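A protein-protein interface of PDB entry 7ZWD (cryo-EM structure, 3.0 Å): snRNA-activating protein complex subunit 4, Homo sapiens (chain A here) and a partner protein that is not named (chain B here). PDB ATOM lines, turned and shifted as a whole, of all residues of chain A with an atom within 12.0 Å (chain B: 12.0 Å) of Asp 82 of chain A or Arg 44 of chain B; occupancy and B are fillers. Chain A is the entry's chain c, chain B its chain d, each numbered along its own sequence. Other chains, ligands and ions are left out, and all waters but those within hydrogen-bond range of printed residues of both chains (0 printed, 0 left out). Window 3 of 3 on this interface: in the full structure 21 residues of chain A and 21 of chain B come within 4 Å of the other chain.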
ATOM      1  N   GLU A  81       9.654   7.985 -22.220  1.00  0.00           N
ATOM      2  CA  GLU A  81       9.508   9.271 -22.890  1.00  0.00           C
ATOM      3  C   GLU A  81       8.537  10.190 -22.140  1.00  0.00           C
ATOM      4  O   GLU A  81       8.959  11.037 -21.352  1.00  0.00           O
ATOM      5  CB  GLU A  81       9.067   9.070 -24.352  1.00  0.00           C
ATOM      6  CG  GLU A  81       7.955   8.039 -24.602  1.00  0.00           C
ATOM      7  CD  GLU A  81       8.454   6.604 -24.604  1.00  0.00           C
ATOM      8  OE1 GLU A  81       7.630   5.685 -24.801  1.00  0.00           O
ATOM      9  OE2 GLU A  81       9.670   6.392 -24.412  1.00  0.00           O
ATOM     10  N   ASP A  82       7.247  10.019 -22.383  1.00  0.00           N
ATOM     11  CA  ASP A  82       6.193  10.781 -21.735  1.00  0.00           C
ATOM     12  C   ASP A  82       5.093   9.796 -21.369  1.00  0.00           C
ATOM     13  O   ASP A  82       4.611   9.052 -22.230  1.00  0.00           O
ATOM     14  CB  ASP A  82       5.670  11.884 -22.668  1.00  0.00           C
ATOM     15  CG  ASP A  82       4.575  12.737 -22.043  1.00  0.00           C
ATOM     16  OD1 ASP A  82       3.966  13.532 -22.787  1.00  0.00           O
ATOM     17  OD2 ASP A  82       4.331  12.651 -20.826  1.00  0.00           O
ATOM     18  N   PRO A  83       4.684   9.760 -20.097  1.00  0.00           N
ATOM     19  CA  PRO A  83       3.757   8.709 -19.643  1.00  0.00           C
ATOM     20  C   PRO A  83       2.377   8.739 -20.288  1.00  0.00           C
ATOM     21  O   PRO A  83       1.506   7.973 -19.860  1.00  0.00           O
ATOM     22  CB  PRO A  83       3.662   8.962 -18.133  1.00  0.00           C
ATOM     23  CG  PRO A  83       4.947   9.626 -17.788  1.00  0.00           C
ATOM     24  CD  PRO A  83       5.288  10.485 -18.966  1.00  0.00           C
ATOM     25  N   GLU A  84       2.129   9.597 -21.280  1.00  0.00           N
ATOM     26  CA  GLU A  84       0.866   9.531 -22.010  1.00  0.00           C
ATOM     27  C   GLU A  84       0.726   8.190 -22.727  1.00  0.00           C
ATOM     28  O   GLU A  84      -0.368   7.607 -22.785  1.00  0.00           O
ATOM     29  CB  GLU A  84       0.775  10.694 -23.001  1.00  0.00           C
ATOM     30  CG  GLU A  84       1.163  12.071 -22.444  1.00  0.00           C
ATOM     31  CD  GLU A  84       0.658  12.340 -21.035  1.00  0.00           C
ATOM     32  OE1 GLU A  84       1.397  12.980 -20.257  1.00  0.00           O
ATOM     33  OE2 GLU A  84      -0.489  11.962 -20.717  1.00  0.00           O
ATOM     34  N   THR A  85       1.832   7.681 -23.279  1.00  0.00           N
ATOM     35  CA  THR A  85       1.810   6.341 -23.856  1.00  0.00           C
ATOM     36  C   THR A  85       1.570   5.284 -22.786  1.00  0.00           C
ATOM     37  O   THR A  85       0.916   4.267 -23.055  1.00  0.00           O
ATOM     38  CB  THR A  85       3.114   6.055 -24.610  1.00  0.00           C
ATOM     39  OG1 THR A  85       3.111   4.699 -25.072  1.00  0.00           O
ATOM     40  CG2 THR A  85       4.322   6.273 -23.713  1.00  0.00           C
ATOM     41  N   CYS A  86       2.072   5.515 -21.569  1.00  0.00           N
ATOM     42  CA  CYS A  86       1.735   4.636 -20.455  1.00  0.00           C
ATOM     43  C   CYS A  86       0.233   4.619 -20.219  1.00  0.00           C
ATOM     44  O   CYS A  86      -0.366   3.546 -20.076  1.00  0.00           O
ATOM     45  CB  CYS A  86       2.472   5.073 -19.190  1.00  0.00           C
ATOM     46  SG  CYS A  86       2.693   3.763 -17.966  1.00  0.00           S
ATOM     47  N   LEU A  87      -0.389   5.801 -20.195  1.00  0.00           N
ATOM     48  CA  LEU A  87      -1.838   5.869 -20.048  1.00  0.00           C
ATOM     49  C   LEU A  87      -2.536   5.057 -21.125  1.00  0.00           C
ATOM     50  O   LEU A  87      -3.387   4.219 -20.818  1.00  0.00           O
ATOM     51  CB  LEU A  87      -2.332   7.315 -20.101  1.00  0.00           C
ATOM     52  CG  LEU A  87      -1.624   8.463 -19.391  1.00  0.00           C
ATOM     53  CD1 LEU A  87      -2.413   9.730 -19.623  1.00  0.00           C
ATOM     54  CD2 LEU A  87      -1.519   8.177 -17.913  1.00  0.00           C
ATOM     55  N   GLN A  88      -2.186   5.279 -22.395  1.00  0.00           N
ATOM     56  CA  GLN A  88      -2.963   4.654 -23.464  1.00  0.00           C
ATOM     57  C   GLN A  88      -2.770   3.137 -23.487  1.00  0.00           C
ATOM     58  O   GLN A  88      -3.733   2.386 -23.701  1.00  0.00           O
ATOM     59  CB  GLN A  88      -2.628   5.279 -24.824  1.00  0.00           C
ATOM     60  CG  GLN A  88      -1.169   5.264 -25.245  1.00  0.00           C
ATOM     61  CD  GLN A  88      -0.723   3.937 -25.834  1.00  0.00           C
ATOM     62  OE1 GLN A  88      -1.544   3.131 -26.274  1.00  0.00           O
ATOM     63  NE2 GLN A  88       0.584   3.705 -25.846  1.00  0.00           N
ATOM     64  N   LEU A  89      -1.544   2.657 -23.242  1.00  0.00           N
ATOM     65  CA  LEU A  89      -1.334   1.214 -23.281  1.00  0.00           C
ATOM     66  C   LEU A  89      -1.954   0.538 -22.062  1.00  0.00           C
ATOM     67  O   LEU A  89      -2.527  -0.554 -22.174  1.00  0.00           O
ATOM     68  CB  LEU A  89       0.157   0.885 -23.393  1.00  0.00           C
ATOM     69  CG  LEU A  89       0.533  -0.596 -23.245  1.00  0.00           C
ATOM     70  CD1 LEU A  89      -0.269  -1.450 -24.216  1.00  0.00           C
ATOM     71  CD2 LEU A  89       2.015  -0.823 -23.475  1.00  0.00           C
ATOM     72  N   ASN A  90      -1.881   1.175 -20.891  1.00  0.00           N
ATOM     73  CA  ASN A  90      -2.563   0.610 -19.734  1.00  0.00           C
ATOM     74  C   ASN A  90      -4.073   0.626 -19.934  1.00  0.00           C
ATOM     75  O   ASN A  90      -4.770  -0.283 -19.479  1.00  0.00           O
ATOM     76  CB  ASN A  90      -2.168   1.357 -18.461  1.00  0.00           C
ATOM     77  CG  ASN A  90      -2.073   0.436 -17.260  1.00  0.00           C
ATOM     78  OD1 ASN A  90      -1.349  -0.557 -17.285  1.00  0.00           O
ATOM     79  ND2 ASN A  90      -2.805   0.760 -16.203  1.00  0.00           N
ATOM     80  N   MET A  91      -4.594   1.634 -20.642  1.00  0.00           N
ATOM     81  CA  MET A  91      -6.024   1.667 -20.934  1.00  0.00           C
ATOM     82  C   MET A  91      -6.435   0.542 -21.873  1.00  0.00           C
ATOM     83  O   MET A  91      -7.482  -0.079 -21.672  1.00  0.00           O
ATOM     84  CB  MET A  91      -6.429   3.024 -21.522  1.00  0.00           C
ATOM     85  CG  MET A  91      -6.375   4.210 -20.559  1.00  0.00           C
ATOM     86  SD  MET A  91      -7.303   4.051 -19.013  1.00  0.00           S
ATOM     87  CE  MET A  91      -8.808   3.236 -19.553  1.00  0.00           C
ATOM     88  N   GLU B  33      -3.178   3.407 -12.708  1.00  0.00           N
ATOM     89  CA  GLU B  33      -3.731   4.517 -13.483  1.00  0.00           C
ATOM     90  C   GLU B  33      -3.769   5.802 -12.667  1.00  0.00           C
ATOM     91  O   GLU B  33      -3.376   6.868 -13.156  1.00  0.00           O
ATOM     92  CB  GLU B  33      -5.132   4.174 -13.997  1.00  0.00           C
ATOM     93  CG  GLU B  33      -5.223   2.898 -14.816  1.00  0.00           C
ATOM     94  CD  GLU B  33      -4.772   3.074 -16.257  1.00  0.00           C
ATOM     95  OE1 GLU B  33      -3.800   3.816 -16.510  1.00  0.00           O
ATOM     96  OE2 GLU B  33      -5.390   2.450 -17.143  1.00  0.00           O
ATOM     97  N   LEU B  34      -4.264   5.727 -11.428  1.00  0.00           N
ATOM     98  CA  LEU B  34      -4.266   6.908 -10.566  1.00  0.00           C
ATOM     99  C   LEU B  34      -2.848   7.410 -10.312  1.00  0.00           C
ATOM    100  O   LEU B  34      -2.609   8.626 -10.286  1.00  0.00           O
ATOM    101  CB  LEU B  34      -4.975   6.613  -9.243  1.00  0.00           C
ATOM    102  CG  LEU B  34      -6.297   5.844  -9.271  1.00  0.00           C
ATOM    103  CD1 LEU B  34      -6.867   5.703  -7.867  1.00  0.00           C
ATOM    104  CD2 LEU B  34      -7.299   6.525 -10.191  1.00  0.00           C
ATOM    105  N   ALA B  35      -1.896   6.492 -10.122  1.00  0.00           N
ATOM    106  CA  ALA B  35      -0.504   6.903  -9.952  1.00  0.00           C
ATOM    107  C   ALA B  35       0.011   7.637 -11.186  1.00  0.00           C
ATOM    108  O   ALA B  35       0.702   8.659 -11.072  1.00  0.00           O
ATOM    109  CB  ALA B  35       0.368   5.686  -9.645  1.00  0.00           C
ATOM    110  N   LEU B  36      -0.320   7.128 -12.378  1.00  0.00           N
ATOM    111  CA  LEU B  36       0.073   7.794 -13.614  1.00  0.00           C
ATOM    112  C   LEU B  36      -0.535   9.181 -13.719  1.00  0.00           C
ATOM    113  O   LEU B  36       0.160  10.125 -14.100  1.00  0.00           O
ATOM    114  CB  LEU B  36      -0.345   6.972 -14.838  1.00  0.00           C
ATOM    115  CG  LEU B  36       0.018   5.498 -15.000  1.00  0.00           C
ATOM    116  CD1 LEU B  36      -0.271   5.032 -16.413  1.00  0.00           C
ATOM    117  CD2 LEU B  36       1.470   5.274 -14.655  1.00  0.00           C
ATOM    118  N   GLN B  37      -1.825   9.319 -13.402  1.00  0.00           N
ATOM    119  CA  GLN B  37      -2.463  10.632 -13.459  1.00  0.00           C
ATOM    120  C   GLN B  37      -1.776  11.609 -12.514  1.00  0.00           C
ATOM    121  O   GLN B  37      -1.480  12.752 -12.889  1.00  0.00           O
ATOM    122  CB  GLN B  37      -3.955  10.522 -13.127  1.00  0.00           C
ATOM    123  CG  GLN B  37      -4.749   9.464 -13.897  1.00  0.00           C
ATOM    124  CD  GLN B  37      -4.260   9.225 -15.318  1.00  0.00           C
ATOM    125  OE1 GLN B  37      -4.020  10.165 -16.077  1.00  0.00           O
ATOM    126  NE2 GLN B  37      -4.104   7.957 -15.681  1.00  0.00           N
ATOM    127  N   SER B  38      -1.499  11.165 -11.285  1.00  0.00           N
ATOM    128  CA  SER B  38      -0.815  12.021 -10.323  1.00  0.00           C
ATOM    129  C   SER B  38       0.543  12.469 -10.852  1.00  0.00           C
ATOM    130  O   SER B  38       0.873  13.664 -10.826  1.00  0.00           O
ATOM    131  CB  SER B  38      -0.658  11.289  -8.989  1.00  0.00           C
ATOM    132  OG  SER B  38       0.384  10.332  -9.052  1.00  0.00           O
ATOM    133  N   MET B  39       1.338  11.527 -11.369  1.00  0.00           N
ATOM    134  CA  MET B  39       2.697  11.895 -11.750  1.00  0.00           C
ATOM    135  C   MET B  39       2.711  12.730 -13.025  1.00  0.00           C
ATOM    136  O   MET B  39       3.574  13.599 -13.186  1.00  0.00           O
ATOM    137  CB  MET B  39       3.584  10.660 -11.913  1.00  0.00           C
ATOM    138  CG  MET B  39       3.179   9.685 -12.994  1.00  0.00           C
ATOM    139  SD  MET B  39       4.652   8.808 -13.559  1.00  0.00           S
ATOM    140  CE  MET B  39       3.968   7.724 -14.800  1.00  0.00           C
ATOM    141  N   ILE B  40       1.763  12.507 -13.940  1.00  0.00           N
ATOM    142  CA  ILE B  40       1.755  13.327 -15.148  1.00  0.00           C
ATOM    143  C   ILE B  40       1.275  14.731 -14.823  1.00  0.00           C
ATOM    144  O   ILE B  40       1.753  15.707 -15.407  1.00  0.00           O
ATOM    145  CB  ILE B  40       0.913  12.695 -16.273  1.00  0.00           C
ATOM    146  CG1 ILE B  40      -0.531  12.479 -15.830  1.00  0.00           C
ATOM    147  CG2 ILE B  40       1.537  11.391 -16.728  1.00  0.00           C
ATOM    148  CD1 ILE B  40      -1.384  11.801 -16.864  1.00  0.00           C
ATOM    149  N   SER B  41       0.332  14.869 -13.886  1.00  0.00           N
ATOM    150  CA  SER B  41      -0.021  16.206 -13.423  1.00  0.00           C
ATOM    151  C   SER B  41       1.197  16.900 -12.826  1.00  0.00           C
ATOM    152  O   SER B  41       1.477  18.067 -13.130  1.00  0.00           O
ATOM    153  CB  SER B  41      -1.159  16.130 -12.405  1.00  0.00           C
ATOM    154  OG  SER B  41      -0.926  15.105 -11.455  1.00  0.00           O
ATOM    155  N   SER B  42       1.961  16.172 -12.005  1.00  0.00           N
ATOM    156  CA  SER B  42       3.147  16.759 -11.389  1.00  0.00           C
ATOM    157  C   SER B  42       4.191  17.151 -12.431  1.00  0.00           C
ATOM    158  O   SER B  42       4.872  18.172 -12.279  1.00  0.00           O
ATOM    159  CB  SER B  42       3.746  15.786 -10.375  1.00  0.00           C
ATOM    160  OG  SER B  42       4.418  14.722 -11.027  1.00  0.00           O
ATOM    161  N   ARG B  43       4.336  16.356 -13.494  1.00  0.00           N
ATOM    162  CA  ARG B  43       5.379  16.617 -14.479  1.00  0.00           C
ATOM    163  C   ARG B  43       4.986  17.662 -15.519  1.00  0.00           C
ATOM    164  O   ARG B  43       5.854  18.424 -15.956  1.00  0.00           O
ATOM    165  CB  ARG B  43       5.803  15.319 -15.172  1.00  0.00           C
ATOM    166  CG  ARG B  43       6.603  14.391 -14.267  1.00  0.00           C
ATOM    167  CD  ARG B  43       6.340  12.924 -14.553  1.00  0.00           C
ATOM    168  NE  ARG B  43       7.131  12.447 -15.683  1.00  0.00           N
ATOM    169  CZ  ARG B  43       7.430  11.170 -15.900  1.00  0.00           C
ATOM    170  NH1 ARG B  43       7.009  10.235 -15.060  1.00  0.00           N
ATOM    171  NH2 ARG B  43       8.157  10.830 -16.956  1.00  0.00           N
ATOM    172  N   ARG B  44       3.716  17.724 -15.929  1.00  0.00           N
ATOM    173  CA  ARG B  44       3.286  18.853 -16.749  1.00  0.00           C
ATOM    174  C   ARG B  44       3.232  20.134 -15.931  1.00  0.00           C
ATOM    175  O   ARG B  44       3.307  21.232 -16.495  1.00  0.00           O
ATOM    176  CB  ARG B  44       1.927  18.587 -17.403  1.00  0.00           C
ATOM    177  CG  ARG B  44       1.726  17.198 -17.994  1.00  0.00           C
ATOM    178  CD  ARG B  44       2.588  16.967 -19.222  1.00  0.00           C
ATOM    179  NE  ARG B  44       3.854  16.324 -18.885  1.00  0.00           N
ATOM    180  CZ  ARG B  44       4.001  15.015 -18.704  1.00  0.00           C
ATOM    181  NH1 ARG B  44       2.958  14.206 -18.834  1.00  0.00           N
ATOM    182  NH2 ARG B  44       5.189  14.513 -18.397  1.00  0.00           N
ATOM    183  N   GLY B  45       3.116  20.020 -14.604  1.00  0.00           N
ATOM    184  CA  GLY B  45       3.253  21.190 -13.757  1.00  0.00           C
ATOM    185  C   GLY B  45       4.617  21.843 -13.834  1.00  0.00           C
ATOM    186  O   GLY B  45       4.772  22.988 -13.396  1.00  0.00           O
ATOM    187  N   ASP B  46       5.614  21.144 -14.382  1.00  0.00           N
ATOM    188  CA  ASP B  46       6.967  21.664 -14.512  1.00  0.00           C
ATOM    189  C   ASP B  46       7.204  22.370 -15.845  1.00  0.00           C
ATOM    190  O   ASP B  46       8.306  22.878 -16.080  1.00  0.00           O
ATOM    191  CB  ASP B  46       7.988  20.540 -14.323  1.00  0.00           C
ATOM    192  CG  ASP B  46       7.722  19.714 -13.079  1.00  0.00           C
ATOM    193  OD1 ASP B  46       7.564  20.311 -11.994  1.00  0.00           O
ATOM    194  OD2 ASP B  46       7.683  18.470 -13.183  1.00  0.00           O
ATOM    195  N   GLU B  47       6.198  22.414 -16.722  1.00  0.00           N
ATOM    196  CA  GLU B  47       6.306  23.180 -17.958  1.00  0.00           C
ATOM    197  C   GLU B  47       5.248  24.262 -18.110  1.00  0.00           C
ATOM    198  O   GLU B  47       5.245  24.945 -19.139  1.00  0.00           O
ATOM    199  CB  GLU B  47       6.252  22.261 -19.190  1.00  0.00           C
ATOM    200  CG  GLU B  47       4.975  21.464 -19.347  1.00  0.00           C
ATOM    201  CD  GLU B  47       5.231  19.973 -19.335  1.00  0.00           C
ATOM    202  OE1 GLU B  47       6.078  19.521 -18.536  1.00  0.00           O
ATOM    203  OE2 GLU B  47       4.597  19.252 -20.134  1.00  0.00           O
ATOM    204  N   MET B  48       4.354  24.439 -17.139  1.00  0.00           N
ATOM    205  CA  MET B  48       3.465  25.590 -17.117  1.00  0.00           C
ATOM    206  C   MET B  48       4.072  26.781 -16.391  1.00  0.00           C
ATOM    207  O   MET B  48       3.394  27.800 -16.222  1.00  0.00           O
ATOM    208  CB  MET B  48       2.120  25.230 -16.475  1.00  0.00           C
ATOM    209  CG  MET B  48       1.422  24.020 -17.075  1.00  0.00           C
ATOM    210  SD  MET B  48       0.208  23.318 -15.940  1.00  0.00           S
ATOM    211  CE  MET B  48       0.110  21.629 -16.523  1.00  0.00           C
ATOM    212  N   LEU B  49       5.328  26.679 -15.959  1.00  0.00           N
ATOM    213  CA  LEU B  49       6.030  27.785 -15.320  1.00  0.00           C
ATOM    214  C   LEU B  49       6.440  28.871 -16.308  1.00  0.00           C
ATOM    215  O   LEU B  49       6.889  29.940 -15.882  1.00  0.00           O
ATOM    216  CB  LEU B  49       7.266  27.267 -14.578  1.00  0.00           C
ATOM    217  CG  LEU B  49       7.129  25.943 -13.822  1.00  0.00           C
ATOM    218  CD1 LEU B  49       8.431  25.594 -13.117  1.00  0.00           C
ATOM    219  CD2 LEU B  49       5.983  26.008 -12.821  1.00  0.00           C
ATOM    220  N   SER B  50       6.296  28.619 -17.608  1.00  0.00           N
ATOM    221  CA  SER B  50       6.592  29.607 -18.642  1.00  0.00           C
ATOM    222  C   SER B  50       5.479  29.538 -19.677  1.00  0.00           C
ATOM    223  O   SER B  50       5.500  28.669 -20.555  1.00  0.00           O
ATOM    224  CB  SER B  50       7.956  29.350 -19.283  1.00  0.00           C
ATOM    225  OG  SER B  50       8.130  27.976 -19.579  1.00  0.00           O
ATOM    226  N   SER B  51       4.514  30.448 -19.575  1.00  0.00           N
ATOM    227  CA  SER B  51       3.367  30.458 -20.470  1.00  0.00           C
ATOM    228  C   SER B  51       3.033  31.903 -20.819  1.00  0.00           C
ATOM    229  O   SER B  51       3.684  32.844 -20.355  1.00  0.00           O
ATOM    230  CB  SER B  51       2.168  29.742 -19.839  1.00  0.00           C
ATOM    231  OG  SER B  51       2.404  28.349 -19.733  1.00  0.00           O
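Of the 19 printed residues of chain B, 7 touch a printed residue of chain A. Of the 11 printed residues of chain A, 7 touch a printed residue of chain B. Hydrophobic or aromatic side chains of chain A within 4 Å of the printed part of chain B: Pro 83, Leu 87 and Met 91. Among the printed residues, 12 pairs touch across the chains.
The side-chain amide nitrogen of Gln 37 of chain B is in hydrogen-bond range of the backbone carbonyl oxygen of Glu 33 of chain B (2.8 Å). The side-chain hydroxyl (OG) of Ser 41 of chain B is in hydrogen-bond range of the backbone carbonyl oxygen (O) of Gln 37 of chain B (2.8 Å). O of Met 39 of chain B lies within hydrogen-bond range of OG of Ser 42 of chain B (2.6 Å). NH1 of Arg 43 of chain B sits at hydrogen-bond distance from SD of Met 39 of chain B, 3.1 Å away. NE of Arg 44 of chain B lies within salt-bridge range of OE2 of Glu 47 of chain B (3.3 Å).
Among the printed residues, pairs that only touch across the chains: Leu 87 of chain A with Gln 37 of chain B (3.4 Å), Pro 83 of chain A with Arg 43 of chain B (3.5 Å), Leu 87 of chain A with Leu 36 of chain B (3.5 Å), Pro 83 of chain A with Ile 40 of chain B (3.5 Å), Pro 83 of chain A with Met 39 of chain B (3.6 Å), Cys 86 of chain A with Leu 36 of chain B (3.6 Å), Leu 87 of chain A with Ile 40 of chain B (3.6 Å) and Glu 84 of chain A with Ile 40 of chain B (3.9 Å).
Asp 82 of chain A touches one residue of chain B. Arg 44 of chain B touches just these residues of chain A: Asp 82 (2.9 Å) and Glu 84 (2.4 Å). Pro 83 of chain A touches three residues of chain B. No residue of chain A comes within 4 Å of Ser 41 of chain B. No residue of chain A comes within 4 Å of Asp 46 of chain B. No residue of chain A comes within 4 Å of Glu 47 of chain B. Met 48 of chain B touches none of the printed residues of chain A. Of the printed residues of chain A, Glu 33 of chain B touches Asn 90 and Met 91. Of the printed residues of chain B, Met 91 of chain A touches Glu 33. Printed residues of chain A within 4 Å of Met 39 of chain B: Pro 83 (3.6 Å). The nearest residue of chain B that does not touch Asp 82 of chain A is Ile 40 of chain B (5.1 Å).
The guanidinium group (NH1) of Arg 44 of chain B is in salt-bridge range of the side-chain carboxylate (OD2) of Asp 82 of chain A. The guanidinium group (NH1) of Arg 44 of chain B lies within salt-bridge range of the side-chain carboxylate (OE1) of Glu 84 of chain A, at 2.4 Å. ND2 of Asn 90 of chain A lies close to OE2 of Glu 33 of chain B (3.2 Å). The side-chain carboxylate (OE2) of Glu 33 of chain B sits close to the side-chain sulfur (SD) of Met 91 of chain A (3.1 Å).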
